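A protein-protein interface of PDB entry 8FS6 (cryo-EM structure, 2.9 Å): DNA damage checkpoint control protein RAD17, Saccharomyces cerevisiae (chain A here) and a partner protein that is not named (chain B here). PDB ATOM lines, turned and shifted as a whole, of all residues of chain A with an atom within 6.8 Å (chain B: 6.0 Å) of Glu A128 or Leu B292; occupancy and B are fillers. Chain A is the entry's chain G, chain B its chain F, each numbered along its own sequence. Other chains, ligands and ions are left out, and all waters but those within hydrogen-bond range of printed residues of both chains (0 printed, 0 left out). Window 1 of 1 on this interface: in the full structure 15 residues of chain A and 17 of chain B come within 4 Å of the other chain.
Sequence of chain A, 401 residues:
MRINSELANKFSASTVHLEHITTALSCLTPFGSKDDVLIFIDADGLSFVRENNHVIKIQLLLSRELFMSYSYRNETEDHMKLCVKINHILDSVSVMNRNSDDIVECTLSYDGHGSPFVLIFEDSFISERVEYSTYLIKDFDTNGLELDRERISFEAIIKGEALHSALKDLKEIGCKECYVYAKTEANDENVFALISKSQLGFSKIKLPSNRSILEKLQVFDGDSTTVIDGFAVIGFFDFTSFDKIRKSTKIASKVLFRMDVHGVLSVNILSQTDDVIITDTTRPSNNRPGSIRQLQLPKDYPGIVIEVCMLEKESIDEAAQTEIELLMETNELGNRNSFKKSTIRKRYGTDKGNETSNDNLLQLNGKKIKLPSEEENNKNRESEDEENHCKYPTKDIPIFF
The side-chain amide nitrogen (ND2) of Asn B286 sits close to a ring nitrogen (ND1) of His B291, 3.1 Å away.
The guanidinium group (NH2) of Arg A129 is in salt-bridge range of the side-chain carboxylate (OE2) of Glu A131.
The backbone NH (N) of Ile B294 lies within hydrogen-bond range of the backbone carbonyl oxygen (O) of Ile B283, 2.7 Å away.
OH of Tyr B256 lies within hydrogen-bond range of NH2 of Arg B255 (2.8 Å).
The backbone carbonyl oxygen (O) of Val B285 is in hydrogen-bond range of the backbone NH (N) of Leu B292 (2.6 Å).
The side-chain sulfur (SG) of Cys B295 sits at hydrogen-bond distance from the side-chain carboxylate (OE2) of Glu B293 (3.1 Å).
Hydrophobic or aromatic side chains of chain A that line the printed part of chain B: Val A95, Ile A126 and Val A130.
Of the 14 printed residues of chain B, 9 touch a printed residue of chain A.
Printed residues of chain B that touch a printed residue of chain A: Arg B252, Arg B255, Tyr B256, Trp B290, His B291, Leu B292, Glu B293, Ile B294 and Cys B295.
Among the printed residues, 20 pairs touch across the chains.
Among the printed residues, Asp or Glu carboxylates within 4 Å of a Lys or Arg side-chain nitrogen of the other chain: Glu A128 with Arg B255 (3.98 Å).
Printed residues of chain B within 4 Å of Ser A92: Arg B255.
Printed residues of chain B within 4 Å of Val A95: Arg B252 (3.4 Å) and Arg B255 (3.3 Å).
Of the printed residues of chain B, Glu A128 touches Arg B252 (3.96 Å), Arg B255 (3.98 Å), Tyr B256 (3.3 Å), Leu B292 (3.3 Å) and Ile B294 (3.6 Å).
Of the printed residues of chain B, Glu A131 touches Trp B290 (3.2 Å) and His B291 (3.1 Å).
Of the printed residues of chain A, Trp B290 touches Val A130 (3.5 Å) and Glu A131 (3.2 Å).
Leu B292 touches three residues of chain A.
The nearest printed residue of chain B that does not touch Glu A128 is Glu B293 (4.3 Å).
The nearest residue of chain A that does not touch Leu B292 is Glu A131 (5.0 Å).
The nearest printed residue of chain A that does not touch Ile B294 is Ser A127 (4.3 Å).
Among the printed residues, merely in contact across the chains: Glu A131 with Trp B290, Val A130 with Tyr B256, Glu A128 with Leu B292, Val A95 with Arg B255, Val A95 with Arg B252, Ile A126 with Cys B295, Val A130 with Leu B292, Arg A129 with Leu B292, Val A130 with Trp B290, Glu A128 with Ile B294, Arg A129 with His B291, Val A130 with His B291, Glu A128 with Arg B252 and Asp A123 with Arg B252.
The backbone carbonyl oxygen (O) of Glu A131 lies within hydrogen-bond range of the backbone NH (N) of His B291 (3.1 Å).
OE2 of Glu A128 sits at hydrogen-bond distance from OH of Tyr B256, at 3.3 Å.
The side-chain carboxylate of Glu A128 is in salt-bridge range of the guanidinium group of Arg B255.
The backbone NH (N) of Glu B293 lies within hydrogen-bond range of the backbone carbonyl oxygen (O) of Arg A129.
O of Ser A92 lies within hydrogen-bond range of NH2 of Arg B255.
The side-chain sulfur (SG) of Cys B295 lies within hydrogen-bond range of the backbone carbonyl oxygen (O) of Ser A127 (3.3 Å).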
ATOM      1  N   SER A  92      -1.587  -5.681 -30.874  1.00  0.00           N
ATOM      2  CA  SER A  92      -1.723  -6.885 -30.059  1.00  0.00           C
ATOM      3  C   SER A  92      -3.028  -6.884 -29.270  1.00  0.00           C
ATOM      4  O   SER A  92      -3.779  -7.866 -29.296  1.00  0.00           O
ATOM      5  CB  SER A  92      -0.530  -7.018 -29.115  1.00  0.00           C
ATOM      6  OG  SER A  92      -0.475  -5.931 -28.209  1.00  0.00           O
ATOM      7  N   VAL A  95      -7.707  -7.698 -29.642  1.00  0.00           N
ATOM      8  CA  VAL A  95      -8.302  -9.025 -29.764  1.00  0.00           C
ATOM      9  C   VAL A  95      -9.824  -8.954 -29.791  1.00  0.00           C
ATOM     10  O   VAL A  95     -10.477  -9.929 -30.189  1.00  0.00           O
ATOM     11  CB  VAL A  95      -7.820  -9.928 -28.615  1.00  0.00           C
ATOM     12  CG1 VAL A  95      -8.021 -11.401 -28.952  1.00  0.00           C
ATOM     13  CG2 VAL A  95      -6.361  -9.650 -28.303  1.00  0.00           C
ATOM     14  N   LEU A 119       3.448  -9.678 -23.245  1.00  0.00           N
ATOM     15  CA  LEU A 119       1.994  -9.579 -23.353  1.00  0.00           C
ATOM     16  C   LEU A 119       1.454 -10.975 -23.649  1.00  0.00           C
ATOM     17  O   LEU A 119       1.295 -11.358 -24.811  1.00  0.00           O
ATOM     18  CB  LEU A 119       1.586  -8.579 -24.435  1.00  0.00           C
ATOM     19  CG  LEU A 119       1.059  -7.229 -23.946  1.00  0.00           C
ATOM     20  CD1 LEU A 119       2.194  -6.374 -23.411  1.00  0.00           C
ATOM     21  CD2 LEU A 119       0.312  -6.507 -25.055  1.00  0.00           C
ATOM     22  N   ILE A 120       1.172 -11.733 -22.595  1.00  0.00           N
ATOM     23  CA  ILE A 120       0.650 -13.089 -22.726  1.00  0.00           C
ATOM     24  C   ILE A 120      -0.871 -13.021 -22.772  1.00  0.00           C
ATOM     25  O   ILE A 120      -1.507 -12.494 -21.853  1.00  0.00           O
ATOM     26  CB  ILE A 120       1.127 -13.983 -21.571  1.00  0.00           C
ATOM     27  CG1 ILE A 120       2.640 -13.858 -21.388  1.00  0.00           C
ATOM     28  CG2 ILE A 120       0.731 -15.431 -21.812  1.00  0.00           C
ATOM     29  CD1 ILE A 120       3.169 -14.574 -20.164  1.00  0.00           C
ATOM     30  N   PHE A 121      -1.456 -13.550 -23.843  1.00  0.00           N
ATOM     31  CA  PHE A 121      -2.902 -13.605 -24.004  1.00  0.00           C
ATOM     32  C   PHE A 121      -3.351 -15.056 -23.915  1.00  0.00           C
ATOM     33  O   PHE A 121      -2.845 -15.911 -24.650  1.00  0.00           O
ATOM     34  CB  PHE A 121      -3.340 -12.999 -25.341  1.00  0.00           C
ATOM     35  CG  PHE A 121      -3.167 -11.506 -25.425  1.00  0.00           C
ATOM     36  CD1 PHE A 121      -2.826 -10.764 -24.307  1.00  0.00           C
ATOM     37  CD2 PHE A 121      -3.350 -10.846 -26.627  1.00  0.00           C
ATOM     38  CE1 PHE A 121      -2.664  -9.397 -24.391  1.00  0.00           C
ATOM     39  CE2 PHE A 121      -3.191  -9.477 -26.713  1.00  0.00           C
ATOM     40  CZ  PHE A 121      -2.851  -8.752 -25.593  1.00  0.00           C
ATOM     41  N   GLU A 122      -4.296 -15.330 -23.020  1.00  0.00           N
ATOM     42  CA  GLU A 122      -4.775 -16.684 -22.775  1.00  0.00           C
ATOM     43  C   GLU A 122      -6.198 -16.819 -23.298  1.00  0.00           C
ATOM     44  O   GLU A 122      -7.096 -16.090 -22.864  1.00  0.00           O
ATOM     45  CB  GLU A 122      -4.714 -17.026 -21.287  1.00  0.00           C
ATOM     46  CG  GLU A 122      -3.313 -17.306 -20.772  1.00  0.00           C
ATOM     47  CD  GLU A 122      -3.310 -17.855 -19.360  1.00  0.00           C
ATOM     48  OE1 GLU A 122      -4.188 -17.459 -18.564  1.00  0.00           O
ATOM     49  OE2 GLU A 122      -2.430 -18.685 -19.046  1.00  0.00           O
ATOM     50  N   ASP A 123      -6.399 -17.756 -24.220  1.00  0.00           N
ATOM     51  CA  ASP A 123      -7.708 -18.077 -24.778  1.00  0.00           C
ATOM     52  C   ASP A 123      -8.168 -19.454 -24.308  1.00  0.00           C
ATOM     53  O   ASP A 123      -8.685 -20.254 -25.091  1.00  0.00           O
ATOM     54  CB  ASP A 123      -7.683 -18.003 -26.302  1.00  0.00           C
ATOM     55  CG  ASP A 123      -9.067 -17.834 -26.903  1.00  0.00           C
ATOM     56  OD1 ASP A 123     -10.020 -17.566 -26.141  1.00  0.00           O
ATOM     57  OD2 ASP A 123      -9.201 -17.970 -28.138  1.00  0.00           O
ATOM     58  N   ILE A 126      -5.580 -21.583 -25.743  1.00  0.00           N
ATOM     59  CA  ILE A 126      -4.512 -20.909 -26.469  1.00  0.00           C
ATOM     60  C   ILE A 126      -3.795 -19.965 -25.517  1.00  0.00           C
ATOM     61  O   ILE A 126      -4.439 -19.171 -24.823  1.00  0.00           O
ATOM     62  CB  ILE A 126      -5.052 -20.140 -27.691  1.00  0.00           C
ATOM     63  CG1 ILE A 126      -5.542 -21.127 -28.744  1.00  0.00           C
ATOM     64  CG2 ILE A 126      -3.983 -19.228 -28.277  1.00  0.00           C
ATOM     65  CD1 ILE A 126      -4.505 -22.151 -29.093  1.00  0.00           C
ATOM     66  N   SER A 127      -2.465 -20.049 -25.486  1.00  0.00           N
ATOM     67  CA  SER A 127      -1.627 -19.183 -24.657  1.00  0.00           C
ATOM     68  C   SER A 127      -0.537 -18.594 -25.548  1.00  0.00           C
ATOM     69  O   SER A 127       0.563 -19.146 -25.648  1.00  0.00           O
ATOM     70  CB  SER A 127      -1.040 -19.951 -23.477  1.00  0.00           C
ATOM     71  OG  SER A 127      -2.063 -20.457 -22.639  1.00  0.00           O
ATOM     72  N   GLU A 128      -0.845 -17.473 -26.195  1.00  0.00           N
ATOM     73  CA  GLU A 128       0.139 -16.777 -27.008  1.00  0.00           C
ATOM     74  C   GLU A 128       0.968 -15.839 -26.137  1.00  0.00           C
ATOM     75  O   GLU A 128       0.546 -15.429 -25.053  1.00  0.00           O
ATOM     76  CB  GLU A 128      -0.550 -16.004 -28.136  1.00  0.00           C
ATOM     77  CG  GLU A 128      -1.212 -14.699 -27.719  1.00  0.00           C
ATOM     78  CD  GLU A 128      -0.311 -13.496 -27.912  1.00  0.00           C
ATOM     79  OE1 GLU A 128       0.881 -13.695 -28.225  1.00  0.00           O
ATOM     80  OE2 GLU A 128      -0.791 -12.355 -27.749  1.00  0.00           O
ATOM     81  N   ARG A 129       2.160 -15.501 -26.624  1.00  0.00           N
ATOM     82  CA  ARG A 129       3.093 -14.672 -25.872  1.00  0.00           C
ATOM     83  C   ARG A 129       3.865 -13.775 -26.827  1.00  0.00           C
ATOM     84  O   ARG A 129       4.464 -14.261 -27.792  1.00  0.00           O
ATOM     85  CB  ARG A 129       4.058 -15.543 -25.058  1.00  0.00           C
ATOM     86  CG  ARG A 129       5.153 -14.780 -24.336  1.00  0.00           C
ATOM     87  CD  ARG A 129       6.287 -15.712 -23.935  1.00  0.00           C
ATOM     88  NE  ARG A 129       7.314 -15.033 -23.154  1.00  0.00           N
ATOM     89  CZ  ARG A 129       7.390 -15.062 -21.831  1.00  0.00           C
ATOM     90  NH1 ARG A 129       6.510 -15.728 -21.102  1.00  0.00           N
ATOM     91  NH2 ARG A 129       8.375 -14.406 -21.223  1.00  0.00           N
ATOM     92  N   VAL A 130       3.853 -12.472 -26.554  1.00  0.00           N
ATOM     93  CA  VAL A 130       4.573 -11.483 -27.347  1.00  0.00           C
ATOM     94  C   VAL A 130       5.585 -10.796 -26.441  1.00  0.00           C
ATOM     95  O   VAL A 130       5.239 -10.358 -25.338  1.00  0.00           O
ATOM     96  CB  VAL A 130       3.627 -10.444 -27.977  1.00  0.00           C
ATOM     97  CG1 VAL A 130       4.418  -9.463 -28.811  1.00  0.00           C
ATOM     98  CG2 VAL A 130       2.577 -11.119 -28.823  1.00  0.00           C
ATOM     99  N   GLU A 131       6.829 -10.701 -26.906  1.00  0.00           N
ATOM    100  CA  GLU A 131       7.914 -10.092 -26.147  1.00  0.00           C
ATOM    101  C   GLU A 131       8.365  -8.827 -26.864  1.00  0.00           C
ATOM    102  O   GLU A 131       8.743  -8.881 -28.039  1.00  0.00           O
ATOM    103  CB  GLU A 131       9.081 -11.068 -25.992  1.00  0.00           C
ATOM    104  CG  GLU A 131       9.075 -11.847 -24.689  1.00  0.00           C
ATOM    105  CD  GLU A 131      10.167 -12.897 -24.636  1.00  0.00           C
ATOM    106  OE1 GLU A 131      10.891 -13.053 -25.641  1.00  0.00           O
ATOM    107  OE2 GLU A 131      10.302 -13.565 -23.590  1.00  0.00           O
ATOM    108  N   ARG B 252      -4.759 -16.442 -34.958  1.00  0.00           N
ATOM    109  CA  ARG B 252      -4.209 -15.483 -34.001  1.00  0.00           C
ATOM    110  C   ARG B 252      -3.048 -14.695 -34.599  1.00  0.00           C
ATOM    111  O   ARG B 252      -2.942 -13.481 -34.390  1.00  0.00           O
ATOM    112  CB  ARG B 252      -3.766 -16.207 -32.730  1.00  0.00           C
ATOM    113  CG  ARG B 252      -3.287 -15.280 -31.625  1.00  0.00           C
ATOM    114  CD  ARG B 252      -4.064 -15.503 -30.339  1.00  0.00           C
ATOM    115  NE  ARG B 252      -5.476 -15.171 -30.487  1.00  0.00           N
ATOM    116  CZ  ARG B 252      -6.303 -14.943 -29.477  1.00  0.00           C
ATOM    117  NH1 ARG B 252      -5.889 -14.993 -28.221  1.00  0.00           N
ATOM    118  NH2 ARG B 252      -7.576 -14.658 -29.732  1.00  0.00           N
ATOM    119  N   VAL B 253      -2.167 -15.367 -35.343  1.00  0.00           N
ATOM    120  CA  VAL B 253      -1.039 -14.689 -35.973  1.00  0.00           C
ATOM    121  C   VAL B 253      -1.469 -13.757 -37.097  1.00  0.00           C
ATOM    122  O   VAL B 253      -0.705 -12.863 -37.477  1.00  0.00           O
ATOM    123  CB  VAL B 253      -0.021 -15.728 -36.488  1.00  0.00           C
ATOM    124  CG1 VAL B 253      -0.493 -16.345 -37.792  1.00  0.00           C
ATOM    125  CG2 VAL B 253       1.359 -15.106 -36.651  1.00  0.00           C
ATOM    126  N   ARG B 255      -3.747 -11.486 -37.016  1.00  0.00           N
ATOM    127  CA  ARG B 255      -4.197 -10.193 -36.518  1.00  0.00           C
ATOM    128  C   ARG B 255      -3.120  -9.119 -36.615  1.00  0.00           C
ATOM    129  O   ARG B 255      -3.452  -7.936 -36.751  1.00  0.00           O
ATOM    130  CB  ARG B 255      -4.670 -10.347 -35.068  1.00  0.00           C
ATOM    131  CG  ARG B 255      -5.213  -9.088 -34.415  1.00  0.00           C
ATOM    132  CD  ARG B 255      -5.436  -9.319 -32.930  1.00  0.00           C
ATOM    133  NE  ARG B 255      -4.186  -9.570 -32.224  1.00  0.00           N
ATOM    134  CZ  ARG B 255      -4.035 -10.482 -31.272  1.00  0.00           C
ATOM    135  NH1 ARG B 255      -5.033 -11.267 -30.903  1.00  0.00           N
ATOM    136  NH2 ARG B 255      -2.851 -10.612 -30.681  1.00  0.00           N
ATOM    137  N   TYR B 256      -1.846  -9.501 -36.571  1.00  0.00           N
ATOM    138  CA  TYR B 256      -0.744  -8.549 -36.603  1.00  0.00           C
ATOM    139  C   TYR B 256      -0.510  -8.069 -38.029  1.00  0.00           C
ATOM    140  O   TYR B 256      -0.460  -8.876 -38.963  1.00  0.00           O
ATOM    141  CB  TYR B 256       0.527  -9.182 -36.037  1.00  0.00           C
ATOM    142  CG  TYR B 256       0.366  -9.715 -34.630  1.00  0.00           C
ATOM    143  CD1 TYR B 256      -0.077 -11.013 -34.403  1.00  0.00           C
ATOM    144  CD2 TYR B 256       0.647  -8.918 -33.528  1.00  0.00           C
ATOM    145  CE1 TYR B 256      -0.229 -11.503 -33.122  1.00  0.00           C
ATOM    146  CE2 TYR B 256       0.497  -9.399 -32.242  1.00  0.00           C
ATOM    147  CZ  TYR B 256       0.058 -10.692 -32.044  1.00  0.00           C
ATOM    148  OH  TYR B 256      -0.094 -11.178 -30.765  1.00  0.00           O
ATOM    149  N   ILE B 283       3.503 -21.326 -33.081  1.00  0.00           N
ATOM    150  CA  ILE B 283       3.720 -20.289 -34.078  1.00  0.00           C
ATOM    151  C   ILE B 283       4.688 -19.280 -33.476  1.00  0.00           C
ATOM    152  O   ILE B 283       4.346 -18.567 -32.525  1.00  0.00           O
ATOM    153  CB  ILE B 283       2.402 -19.628 -34.497  1.00  0.00           C
ATOM    154  CG1 ILE B 283       1.486 -20.659 -35.158  1.00  0.00           C
ATOM    155  CG2 ILE B 283       2.664 -18.465 -35.433  1.00  0.00           C
ATOM    156  CD1 ILE B 283       0.114 -20.129 -35.496  1.00  0.00           C
ATOM    157  N   ILE B 284       5.899 -19.219 -34.022  1.00  0.00           N
ATOM    158  CA  ILE B 284       6.958 -18.351 -33.521  1.00  0.00           C
ATOM    159  C   ILE B 284       7.308 -17.345 -34.607  1.00  0.00           C
ATOM    160  O   ILE B 284       7.557 -17.727 -35.757  1.00  0.00           O
ATOM    161  CB  ILE B 284       8.195 -19.163 -33.097  1.00  0.00           C
ATOM    162  CG1 ILE B 284       7.916 -19.924 -31.798  1.00  0.00           C
ATOM    163  CG2 ILE B 284       9.410 -18.259 -32.946  1.00  0.00           C
ATOM    164  CD1 ILE B 284       9.088 -20.748 -31.310  1.00  0.00           C
ATOM    165  N   VAL B 285       7.308 -16.064 -34.249  1.00  0.00           N
ATOM    166  CA  VAL B 285       7.720 -14.987 -35.144  1.00  0.00           C
ATOM    167  C   VAL B 285       8.745 -14.159 -34.381  1.00  0.00           C
ATOM    168  O   VAL B 285       8.383 -13.329 -33.541  1.00  0.00           O
ATOM    169  CB  VAL B 285       6.544 -14.123 -35.612  1.00  0.00           C
ATOM    170  CG1 VAL B 285       7.042 -12.962 -36.459  1.00  0.00           C
ATOM    171  CG2 VAL B 285       5.554 -14.961 -36.400  1.00  0.00           C
ATOM    172  N   ASN B 286      10.024 -14.389 -34.660  1.00  0.00           N
ATOM    173  CA  ASN B 286      11.111 -13.666 -34.016  1.00  0.00           C
ATOM    174  C   ASN B 286      11.696 -12.660 -34.997  1.00  0.00           C
ATOM    175  O   ASN B 286      11.991 -13.003 -36.146  1.00  0.00           O
ATOM    176  CB  ASN B 286      12.197 -14.629 -33.530  1.00  0.00           C
ATOM    177  CG  ASN B 286      13.052 -14.035 -32.427  1.00  0.00           C
ATOM    178  OD1 ASN B 286      12.982 -12.838 -32.148  1.00  0.00           O
ATOM    179  ND2 ASN B 286      13.862 -14.873 -31.792  1.00  0.00           N
ATOM    180  N   TRP B 290      11.015  -7.710 -31.615  1.00  0.00           N
ATOM    181  CA  TRP B 290       9.824  -8.313 -31.035  1.00  0.00           C
ATOM    182  C   TRP B 290       9.766  -9.791 -31.395  1.00  0.00           C
ATOM    183  O   TRP B 290      10.240 -10.209 -32.455  1.00  0.00           O
ATOM    184  CB  TRP B 290       8.549  -7.587 -31.488  1.00  0.00           C
ATOM    185  CG  TRP B 290       7.975  -8.076 -32.779  1.00  0.00           C
ATOM    186  CD1 TRP B 290       8.472  -7.861 -34.030  1.00  0.00           C
ATOM    187  CD2 TRP B 290       6.781  -8.850 -32.947  1.00  0.00           C
ATOM    188  NE1 TRP B 290       7.665  -8.458 -34.968  1.00  0.00           N
ATOM    189  CE2 TRP B 290       6.621  -9.073 -34.329  1.00  0.00           C
ATOM    190  CE3 TRP B 290       5.836  -9.379 -32.064  1.00  0.00           C
ATOM    191  CZ2 TRP B 290       5.552  -9.802 -34.848  1.00  0.00           C
ATOM    192  CZ3 TRP B 290       4.777 -10.102 -32.581  1.00  0.00           C
ATOM    193  CH2 TRP B 290       4.643 -10.307 -33.960  1.00  0.00           C
ATOM    194  N   HIS B 291       9.179 -10.630 -30.536  1.00  0.00           N
ATOM    195  CA  HIS B 291       9.192 -12.104 -30.745  1.00  0.00           C
ATOM    196  C   HIS B 291       7.873 -12.763 -30.350  1.00  0.00           C
ATOM    197  O   HIS B 291       7.678 -12.990 -29.144  1.00  0.00           O
ATOM    198  CB  HIS B 291      10.342 -12.729 -29.951  1.00  0.00           C
ATOM    199  CG  HIS B 291      10.308 -14.219 -29.897  1.00  0.00           C
ATOM    200  ND1 HIS B 291      10.907 -15.004 -30.859  1.00  0.00           N
ATOM    201  CD2 HIS B 291       9.764 -15.068 -28.999  1.00  0.00           C
ATOM    202  CE1 HIS B 291      10.733 -16.273 -30.559  1.00  0.00           C
ATOM    203  NE2 HIS B 291      10.032 -16.340 -29.423  1.00  0.00           N
ATOM    204  N   LEU B 292       7.014 -13.086 -31.315  1.00  0.00           N
ATOM    205  CA  LEU B 292       5.759 -13.832 -31.046  1.00  0.00           C
ATOM    206  C   LEU B 292       6.133 -15.277 -30.730  1.00  0.00           C
ATOM    207  O   LEU B 292       7.188 -15.725 -31.211  1.00  0.00           O
ATOM    208  CB  LEU B 292       4.846 -13.780 -32.272  1.00  0.00           C
ATOM    209  CG  LEU B 292       3.474 -14.428 -32.108  1.00  0.00           C
ATOM    210  CD1 LEU B 292       2.659 -13.731 -31.034  1.00  0.00           C
ATOM    211  CD2 LEU B 292       2.721 -14.420 -33.425  1.00  0.00           C
ATOM    212  N   GLU B 293       5.322 -15.969 -29.937  1.00  0.00           N
ATOM    213  CA  GLU B 293       5.553 -17.389 -29.582  1.00  0.00           C
ATOM    214  C   GLU B 293       4.201 -17.960 -29.170  1.00  0.00           C
ATOM    215  O   GLU B 293       4.026 -18.253 -27.975  1.00  0.00           O
ATOM    216  CB  GLU B 293       6.592 -17.493 -28.466  1.00  0.00           C
ATOM    217  CG  GLU B 293       6.985 -18.917 -28.128  1.00  0.00           C
ATOM    218  CD  GLU B 293       6.286 -19.504 -26.914  1.00  0.00           C
ATOM    219  OE1 GLU B 293       5.931 -18.731 -26.005  1.00  0.00           O
ATOM    220  OE2 GLU B 293       6.094 -20.732 -26.884  1.00  0.00           O
ATOM    221  N   ILE B 294       3.267 -18.082 -30.113  1.00  0.00           N
ATOM    222  CA  ILE B 294       1.890 -18.540 -29.774  1.00  0.00           C
ATOM    223  C   ILE B 294       1.950 -20.055 -29.594  1.00  0.00           C
ATOM    224  O   ILE B 294       2.788 -20.682 -30.256  1.00  0.00           O
ATOM    225  CB  ILE B 294       0.815 -18.087 -30.790  1.00  0.00           C
ATOM    226  CG1 ILE B 294       0.130 -19.270 -31.479  1.00  0.00           C
ATOM    227  CG2 ILE B 294       1.365 -17.085 -31.795  1.00  0.00           C
ATOM    228  CD1 ILE B 294      -0.976 -18.857 -32.414  1.00  0.00           C
ATOM    229  N   CYS B 295       1.125 -20.610 -28.707  1.00  0.00           N
ATOM    230  CA  CYS B 295       1.153 -22.057 -28.384  1.00  0.00           C
ATOM    231  C   CYS B 295      -0.241 -22.674 -28.429  1.00  0.00           C
ATOM    232  O   CYS B 295      -1.217 -21.919 -28.282  1.00  0.00           O
ATOM    233  CB  CYS B 295       1.700 -22.283 -26.981  1.00  0.00           C
ATOM    234  SG  CYS B 295       3.037 -21.144 -26.540  1.00  0.00           S
